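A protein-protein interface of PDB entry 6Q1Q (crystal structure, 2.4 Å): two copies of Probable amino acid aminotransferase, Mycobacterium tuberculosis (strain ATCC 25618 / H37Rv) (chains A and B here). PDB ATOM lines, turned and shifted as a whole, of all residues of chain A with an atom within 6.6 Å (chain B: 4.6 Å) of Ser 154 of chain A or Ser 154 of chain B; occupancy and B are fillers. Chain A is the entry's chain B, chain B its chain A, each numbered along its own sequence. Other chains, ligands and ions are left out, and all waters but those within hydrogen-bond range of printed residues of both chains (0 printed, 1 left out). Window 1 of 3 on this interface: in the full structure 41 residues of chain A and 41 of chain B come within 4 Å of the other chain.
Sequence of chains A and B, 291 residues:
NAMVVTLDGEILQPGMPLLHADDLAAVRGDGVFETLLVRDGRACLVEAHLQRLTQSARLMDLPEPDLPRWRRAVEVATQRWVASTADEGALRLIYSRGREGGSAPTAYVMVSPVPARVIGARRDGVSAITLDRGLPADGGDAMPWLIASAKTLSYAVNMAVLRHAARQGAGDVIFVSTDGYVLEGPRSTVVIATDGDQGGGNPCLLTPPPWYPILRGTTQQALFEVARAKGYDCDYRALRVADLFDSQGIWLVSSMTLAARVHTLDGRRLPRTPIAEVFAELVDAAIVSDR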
ATOM      1  N   VAL A  27      -5.406 -25.148   1.213  1.00  0.00           N
ATOM      2  CA  VAL A  27      -5.764 -26.520   1.545  1.00  0.00           C
ATOM      3  C   VAL A  27      -4.534 -27.428   1.565  1.00  0.00           C
ATOM      4  O   VAL A  27      -4.493 -28.406   2.321  1.00  0.00           O
ATOM      5  CB  VAL A  27      -6.837 -27.016   0.558  1.00  0.00           C
ATOM      6  CG1 VAL A  27      -7.003 -28.528   0.626  1.00  0.00           C
ATOM      7  CG2 VAL A  27      -8.166 -26.313   0.829  1.00  0.00           C
ATOM      8  N   ARG A  28      -3.502 -27.113   0.779  1.00  0.00           N
ATOM      9  CA  ARG A  28      -2.338 -27.981   0.669  1.00  0.00           C
ATOM     10  C   ARG A  28      -1.000 -27.260   0.745  1.00  0.00           C
ATOM     11  O   ARG A  28       0.039 -27.927   0.668  1.00  0.00           O
ATOM     12  CB  ARG A  28      -2.371 -28.763  -0.656  1.00  0.00           C
ATOM     13  CG  ARG A  28      -3.626 -29.568  -0.932  1.00  0.00           C
ATOM     14  CD  ARG A  28      -3.321 -31.055  -0.955  1.00  0.00           C
ATOM     15  NE  ARG A  28      -4.533 -31.856  -1.090  1.00  0.00           N
ATOM     16  CZ  ARG A  28      -4.906 -32.809  -0.242  1.00  0.00           C
ATOM     17  NH1 ARG A  28      -4.162 -33.092   0.819  1.00  0.00           N
ATOM     18  NH2 ARG A  28      -6.029 -33.478  -0.462  1.00  0.00           N
ATOM     19  N   GLY A  29      -0.983 -25.938   0.901  1.00  0.00           N
ATOM     20  CA  GLY A  29       0.267 -25.207   0.780  1.00  0.00           C
ATOM     21  C   GLY A  29       0.961 -25.461  -0.539  1.00  0.00           C
ATOM     22  O   GLY A  29       2.193 -25.410  -0.612  1.00  0.00           O
ATOM     23  N   ASP A  30       0.188 -25.736  -1.591  1.00  0.00           N
ATOM     24  CA  ASP A  30       0.707 -26.258  -2.854  1.00  0.00           C
ATOM     25  C   ASP A  30       0.960 -25.089  -3.798  1.00  0.00           C
ATOM     26  O   ASP A  30       0.121 -24.736  -4.628  1.00  0.00           O
ATOM     27  CB  ASP A  30      -0.274 -27.260  -3.446  1.00  0.00           C
ATOM     28  CG  ASP A  30       0.343 -28.110  -4.534  1.00  0.00           C
ATOM     29  OD1 ASP A  30       1.581 -28.080  -4.686  1.00  0.00           O
ATOM     30  OD2 ASP A  30      -0.414 -28.813  -5.237  1.00  0.00           O
ATOM     31  N   GLY A  31       2.140 -24.496  -3.677  1.00  0.00           N
ATOM     32  CA  GLY A  31       2.510 -23.374  -4.518  1.00  0.00           C
ATOM     33  C   GLY A  31       3.916 -22.938  -4.180  1.00  0.00           C
ATOM     34  O   GLY A  31       4.588 -23.533  -3.331  1.00  0.00           O
ATOM     35  N   PHE A  33       6.592 -19.258  -3.799  1.00  0.00           N
ATOM     36  CA  PHE A  33       6.558 -17.837  -3.497  1.00  0.00           C
ATOM     37  C   PHE A  33       7.972 -17.279  -3.464  1.00  0.00           C
ATOM     38  O   PHE A  33       8.958 -18.019  -3.403  1.00  0.00           O
ATOM     39  CB  PHE A  33       5.834 -17.554  -2.173  1.00  0.00           C
ATOM     40  CG  PHE A  33       6.699 -17.699  -0.956  1.00  0.00           C
ATOM     41  CD1 PHE A  33       7.009 -18.951  -0.451  1.00  0.00           C
ATOM     42  CD2 PHE A  33       7.186 -16.576  -0.303  1.00  0.00           C
ATOM     43  CE1 PHE A  33       7.800 -19.082   0.675  1.00  0.00           C
ATOM     44  CE2 PHE A  33       7.976 -16.700   0.824  1.00  0.00           C
ATOM     45  CZ  PHE A  33       8.285 -17.954   1.314  1.00  0.00           C
ATOM     46  N   MET A  60       7.998 -27.640  -9.041  1.00  0.00           N
ATOM     47  CA  MET A  60       6.673 -27.897  -8.498  1.00  0.00           C
ATOM     48  C   MET A  60       5.641 -28.208  -9.576  1.00  0.00           C
ATOM     49  O   MET A  60       4.443 -28.256  -9.275  1.00  0.00           O
ATOM     50  CB  MET A  60       6.218 -26.706  -7.655  1.00  0.00           C
ATOM     51  CG  MET A  60       6.833 -26.674  -6.269  1.00  0.00           C
ATOM     52  SD  MET A  60       5.948 -27.755  -5.133  1.00  0.00           S
ATOM     53  CE  MET A  60       4.524 -26.737  -4.745  1.00  0.00           C
ATOM     54  N   LYS A 151      11.263 -23.233  -3.275  1.00  0.00           N
ATOM     55  CA  LYS A 151      10.768 -22.344  -2.224  1.00  0.00           C
ATOM     56  C   LYS A 151       9.246 -22.357  -2.287  1.00  0.00           C
ATOM     57  O   LYS A 151       8.626 -21.593  -3.026  1.00  0.00           O
ATOM     58  CB  LYS A 151      11.331 -20.939  -2.393  1.00  0.00           C
ATOM     59  CG  LYS A 151      10.924 -19.971  -1.300  1.00  0.00           C
ATOM     60  CD  LYS A 151      11.634 -18.640  -1.466  1.00  0.00           C
ATOM     61  CE  LYS A 151      11.512 -17.788  -0.216  1.00  0.00           C
ATOM     62  NZ  LYS A 151      11.855 -18.552   1.018  1.00  0.00           N
ATOM     63  N   THR A 152       8.638 -23.238  -1.498  1.00  0.00           N
ATOM     64  CA  THR A 152       7.209 -23.500  -1.565  1.00  0.00           C
ATOM     65  C   THR A 152       6.452 -22.787  -0.448  1.00  0.00           C
ATOM     66  O   THR A 152       7.033 -22.238   0.492  1.00  0.00           O
ATOM     67  CB  THR A 152       6.939 -25.006  -1.499  1.00  0.00           C
ATOM     68  OG1 THR A 152       7.083 -25.457  -0.147  1.00  0.00           O
ATOM     69  CG2 THR A 152       7.913 -25.762  -2.394  1.00  0.00           C
ATOM     70  N   LEU A 153       5.125 -22.801  -0.570  1.00  0.00           N
ATOM     71  CA  LEU A 153       4.232 -22.231   0.430  1.00  0.00           C
ATOM     72  C   LEU A 153       4.054 -23.116   1.657  1.00  0.00           C
ATOM     73  O   LEU A 153       3.285 -22.754   2.549  1.00  0.00           O
ATOM     74  CB  LEU A 153       2.858 -21.952  -0.188  1.00  0.00           C
ATOM     75  CG  LEU A 153       2.801 -20.912  -1.305  1.00  0.00           C
ATOM     76  CD1 LEU A 153       1.401 -20.837  -1.880  1.00  0.00           C
ATOM     77  CD2 LEU A 153       3.233 -19.559  -0.778  1.00  0.00           C
ATOM     78  N   SER A 154       4.730 -24.260   1.728  1.00  0.00           N
ATOM     79  CA  SER A 154       4.558 -25.201   2.832  1.00  0.00           C
ATOM     80  C   SER A 154       5.640 -24.946   3.883  1.00  0.00           C
ATOM     81  O   SER A 154       6.645 -25.653   3.974  1.00  0.00           O
ATOM     82  CB  SER A 154       4.578 -26.627   2.308  1.00  0.00           C
ATOM     83  OG  SER A 154       3.334 -26.936   1.702  1.00  0.00           O
ATOM     84  N   TYR A 155       5.410 -23.912   4.694  1.00  0.00           N
ATOM     85  CA  TYR A 155       6.384 -23.420   5.661  1.00  0.00           C
ATOM     86  C   TYR A 155       6.021 -23.761   7.103  1.00  0.00           C
ATOM     87  O   TYR A 155       6.556 -23.146   8.029  1.00  0.00           O
ATOM     88  CB  TYR A 155       6.545 -21.909   5.498  1.00  0.00           C
ATOM     89  CG  TYR A 155       7.838 -21.499   4.834  1.00  0.00           C
ATOM     90  CD1 TYR A 155       8.295 -22.155   3.695  1.00  0.00           C
ATOM     91  CD2 TYR A 155       8.582 -20.430   5.317  1.00  0.00           C
ATOM     92  CE1 TYR A 155       9.474 -21.777   3.078  1.00  0.00           C
ATOM     93  CE2 TYR A 155       9.760 -20.041   4.702  1.00  0.00           C
ATOM     94  CZ  TYR A 155      10.201 -20.720   3.583  1.00  0.00           C
ATOM     95  OH  TYR A 155      11.372 -20.342   2.963  1.00  0.00           O
ATOM     96  N   ALA A 156       5.128 -24.731   7.315  1.00  0.00           N
ATOM     97  CA  ALA A 156       4.694 -25.057   8.672  1.00  0.00           C
ATOM     98  C   ALA A 156       5.865 -25.503   9.542  1.00  0.00           C
ATOM     99  O   ALA A 156       6.005 -25.061  10.690  1.00  0.00           O
ATOM    100  CB  ALA A 156       3.612 -26.137   8.637  1.00  0.00           C
ATOM    101  N   VAL A 157       6.712 -26.389   9.015  1.00  0.00           N
ATOM    102  CA  VAL A 157       7.831 -26.900   9.801  1.00  0.00           C
ATOM    103  C   VAL A 157       8.859 -25.807  10.054  1.00  0.00           C
ATOM    104  O   VAL A 157       9.454 -25.737  11.137  1.00  0.00           O
ATOM    105  CB  VAL A 157       8.456 -28.123   9.109  1.00  0.00           C
ATOM    106  CG1 VAL A 157       9.705 -28.579   9.855  1.00  0.00           C
ATOM    107  CG2 VAL A 157       7.441 -29.251   9.031  1.00  0.00           C
ATOM    108  N   ASN A 158       9.079 -24.931   9.071  1.00  0.00           N
ATOM    109  CA  ASN A 158      10.028 -23.837   9.254  1.00  0.00           C
ATOM    110  C   ASN A 158       9.635 -22.962  10.437  1.00  0.00           C
ATOM    111  O   ASN A 158      10.477 -22.615  11.275  1.00  0.00           O
ATOM    112  CB  ASN A 158      10.128 -23.003   7.976  1.00  0.00           C
ATOM    113  CG  ASN A 158      10.829 -23.739   6.850  1.00  0.00           C
ATOM    114  OD1 ASN A 158      11.929 -24.263   7.025  1.00  0.00           O
ATOM    115  ND2 ASN A 158      10.197 -23.778   5.686  1.00  0.00           N
ATOM    116  N   ARG B  28       1.865 -19.438   4.140  1.00  0.00           N
ATOM    117  CA  ARG B  28       2.840 -20.274   4.825  1.00  0.00           C
ATOM    118  C   ARG B  28       2.386 -21.710   5.048  1.00  0.00           C
ATOM    119  O   ARG B  28       3.150 -22.494   5.621  1.00  0.00           O
ATOM    120  CB  ARG B  28       3.227 -19.654   6.178  1.00  0.00           C
ATOM    121  CG  ARG B  28       3.724 -18.221   6.077  1.00  0.00           C
ATOM    122  CD  ARG B  28       5.199 -18.111   6.428  1.00  0.00           C
ATOM    123  NE  ARG B  28       5.725 -16.779   6.141  1.00  0.00           N
ATOM    124  CZ  ARG B  28       6.758 -16.543   5.339  1.00  0.00           C
ATOM    125  NH1 ARG B  28       7.377 -17.551   4.741  1.00  0.00           N
ATOM    126  NH2 ARG B  28       7.172 -15.300   5.129  1.00  0.00           N
ATOM    127  N   GLY B  29       1.189 -22.085   4.601  1.00  0.00           N
ATOM    128  CA  GLY B  29       0.663 -23.398   4.938  1.00  0.00           C
ATOM    129  C   GLY B  29       0.600 -23.653   6.425  1.00  0.00           C
ATOM    130  O   GLY B  29       0.738 -24.801   6.862  1.00  0.00           O
ATOM    131  N   THR B 152      -0.462 -31.194   9.136  1.00  0.00           N
ATOM    132  CA  THR B 152      -0.471 -29.778   8.813  1.00  0.00           C
ATOM    133  C   THR B 152      -0.963 -29.543   7.391  1.00  0.00           C
ATOM    134  O   THR B 152      -1.076 -30.463   6.577  1.00  0.00           O
ATOM    135  CB  THR B 152       0.927 -29.177   8.978  1.00  0.00           C
ATOM    136  OG1 THR B 152       1.729 -29.531   7.844  1.00  0.00           O
ATOM    137  CG2 THR B 152       1.590 -29.702  10.242  1.00  0.00           C
ATOM    138  N   LEU B 153      -1.239 -28.274   7.096  1.00  0.00           N
ATOM    139  CA  LEU B 153      -1.639 -27.833   5.767  1.00  0.00           C
ATOM    140  C   LEU B 153      -0.464 -27.739   4.805  1.00  0.00           C
ATOM    141  O   LEU B 153      -0.661 -27.352   3.647  1.00  0.00           O
ATOM    142  CB  LEU B 153      -2.327 -26.467   5.855  1.00  0.00           C
ATOM    143  CG  LEU B 153      -3.632 -26.379   6.647  1.00  0.00           C
ATOM    144  CD1 LEU B 153      -4.105 -24.934   6.733  1.00  0.00           C
ATOM    145  CD2 LEU B 153      -4.700 -27.250   6.016  1.00  0.00           C
ATOM    146  N   SER B 154       0.745 -28.086   5.248  1.00  0.00           N
ATOM    147  CA  SER B 154       1.943 -27.952   4.423  1.00  0.00           C
ATOM    148  C   SER B 154       2.212 -29.281   3.721  1.00  0.00           C
ATOM    149  O   SER B 154       3.093 -30.059   4.093  1.00  0.00           O
ATOM    150  CB  SER B 154       3.123 -27.502   5.275  1.00  0.00           C
ATOM    151  OG  SER B 154       3.040 -26.111   5.547  1.00  0.00           O
ATOM    152  N   TYR B 155       1.439 -29.525   2.662  1.00  0.00           N
ATOM    153  CA  TYR B 155       1.442 -30.793   1.943  1.00  0.00           C
ATOM    154  C   TYR B 155       2.118 -30.702   0.579  1.00  0.00           C
ATOM    155  O   TYR B 155       1.902 -31.573  -0.270  1.00  0.00           O
ATOM    156  CB  TYR B 155       0.009 -31.305   1.785  1.00  0.00           C
ATOM    157  CG  TYR B 155      -0.333 -32.458   2.701  1.00  0.00           C
ATOM    158  CD1 TYR B 155      -0.034 -32.406   4.058  1.00  0.00           C
ATOM    159  CD2 TYR B 155      -0.960 -33.596   2.210  1.00  0.00           C
ATOM    160  CE1 TYR B 155      -0.344 -33.459   4.901  1.00  0.00           C
ATOM    161  CE2 TYR B 155      -1.275 -34.656   3.045  1.00  0.00           C
ATOM    162  CZ  TYR B 155      -0.965 -34.581   4.388  1.00  0.00           C
ATOM    163  OH  TYR B 155      -1.275 -35.631   5.226  1.00  0.00           O
ATOM    164  N   ALA B 156       2.930 -29.666   0.346  1.00  0.00           N
ATOM    165  CA  ALA B 156       3.555 -29.494  -0.964  1.00  0.00           C
ATOM    166  C   ALA B 156       4.418 -30.697  -1.322  1.00  0.00           C
ATOM    167  O   ALA B 156       4.335 -31.228  -2.436  1.00  0.00           O
ATOM    168  CB  ALA B 156       4.386 -28.211  -0.992  1.00  0.00           C
ATOM    169  N   ASN B 158       4.181 -33.672  -0.058  1.00  0.00           N
ATOM    170  CA  ASN B 158       3.311 -34.839  -0.160  1.00  0.00           C
ATOM    171  C   ASN B 158       2.774 -34.998  -1.577  1.00  0.00           C
ATOM    172  O   ASN B 158       2.808 -36.095  -2.147  1.00  0.00           O
ATOM    173  CB  ASN B 158       2.167 -34.710   0.846  1.00  0.00           C
ATOM    174  CG  ASN B 158       2.647 -34.801   2.282  1.00  0.00           C
ATOM    175  OD1 ASN B 158       3.345 -33.909   2.770  1.00  0.00           O
ATOM    176  ND2 ASN B 158       2.271 -35.875   2.968  1.00  0.00           N
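Printed residues of chain A within 4 Å of Ser 154 of chain B: Arg 28 (3.98 Å), Ser 154 (3.2 Å), Tyr 155 (3.3 Å) and Ala 156 (3.1 Å). Of the printed residues of chain B, Ala 156 of chain A touches Arg 28, Gly 29, Thr 152 and Ser 154. Of the printed residues of chain B, Leu 153 of chain A touches Arg 28 and Gly 29. Of the printed residues of chain B, Gly 29 of chain A touches Leu 153 (3.1 Å) and Ala 156 (3.6 Å). Of the printed residues of chain B, Arg 28 of chain A touches Leu 153, Ser 154, Tyr 155 and Ala 156. Of the printed residues of chain B, Val 27 of chain A touches Leu 153 (3.9 Å). The nearest printed residue of chain A that does not touch Ser 154 of chain B is Leu 153 of chain A (4.5 Å). The nearest printed residue of chain B that does not touch Val 27 of chain A is Tyr 155 of chain B (5.4 Å).
Among the printed residues, merely in contact across the chains: Ser 154 of chain A with Ser 154 of chain B (3.2 Å), Phe 33 of chain A with Arg 28 of chain B (3.6 Å), Gly 29 of chain A with Ala 156 of chain B (3.6 Å), Ala 156 of chain A with Gly 29 of chain B (3.6 Å), Val 27 of chain A with Leu 153 of chain B (3.9 Å), Ser 154 of chain A with Arg 28 of chain B (3.9 Å), Thr 152 of chain A with Ala 156 of chain B (3.9 Å), Ala 156 of chain A with Thr 152 of chain B (3.96 Å) and Arg 28 of chain A with Ser 154 of chain B (3.98 Å).
N of Ser 154 of chain A sits close to OG1 of Thr 152 of chain A (3.2 Å). The backbone carbonyl oxygen (O) of Gly 31 of chain A is in hydrogen-bond range of the backbone NH (N) of Leu 153 of chain A, at 2.9 Å. OG1 of Thr 152 of chain B lies close to N of Ser 154 of chain B. The side-chain hydroxyl (OG) of Ser 154 of chain A is in hydrogen-bond range of the backbone carbonyl oxygen (O) of Gly 29 of chain A, 3.0 Å away. The side-chain hydroxyl of Tyr 155 of chain A is in hydrogen-bond range of the side-chain amino group of Lys 151 of chain A, 2.7 Å away. O of Gly 29 of chain B lies within hydrogen-bond range of OG of Ser 154 of chain B, at 3.0 Å.
OG of Ser 154 of chain B lies within hydrogen-bond range of N of Tyr 155 of chain A (3.3 Å). O of Arg 28 of chain A lies close to O of Leu 153 of chain B (3.1 Å). O of Arg 28 of chain B sits at hydrogen-bond distance from N of Ala 156 of chain A (3.4 Å). The backbone NH (N) of Gly 29 of chain B sits at hydrogen-bond distance from the backbone carbonyl oxygen (O) of Leu 153 of chain A (3.0 Å). N of Ala 156 of chain B sits at hydrogen-bond distance from O of Arg 28 of chain A (3.4 Å). O of Arg 28 of chain B is in hydrogen-bond range of N of Tyr 155 of chain A (2.8 Å). The backbone carbonyl oxygen (O) of Leu 153 of chain B sits at hydrogen-bond distance from the backbone NH (N) of Gly 29 of chain A, 3.1 Å away. O of Leu 153 of chain A sits close to O of Arg 28 of chain B (3.1 Å). The backbone NH (N) of Ala 156 of chain A sits at hydrogen-bond distance from the side-chain hydroxyl (OG) of Ser 154 of chain B, 3.1 Å away. N of Tyr 155 of chain B is in hydrogen-bond range of OG of Ser 154 of chain A (3.3 Å). The backbone NH (N) of Ala 156 of chain B sits at hydrogen-bond distance from the side-chain hydroxyl (OG) of Ser 154 of chain A (3.1 Å). The backbone NH (N) of Tyr 155 of chain B sits at hydrogen-bond distance from the backbone carbonyl oxygen (O) of Arg 28 of chain A, at 2.9 Å.
Arg 28 of chain A touches Ser 154 of chain B, and with the chains exchanged Ser 154 of chain A touches Arg 28 of chain B. Arg 28 of chain A touches Tyr 155 of chain B, and with the chains exchanged Tyr 155 of chain A touches Arg 28 of chain B. Gly 29 of chain A touches Ala 156 of chain B, and with the chains exchanged Ala 156 of chain A touches Gly 29 of chain B. Ser 154 of chain A touches its own counterpart, Ser 154 of chain B. Positions printed for both chains: 28, 29, 152, 153, 154, 155, 156 and 158. Of the 21 pairs that touch across the chains among the printed residues, 19 have their exchanged pair printed and touching as well.
Printed residues of chain B that touch a printed residue of chain A: Arg 28, Gly 29, Thr 152, Leu 153, Ser 154, Tyr 155 and Ala 156. Hydrophobic or aromatic side chains of chain B that line the printed part of chain A: Leu 153, Tyr 155 and Ala 156. Of the 15 printed residues of chain A, 9 touch a printed residue of chain B. Along chain A the printed residues that touch a printed residue of chain B span positions 27 to 156.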
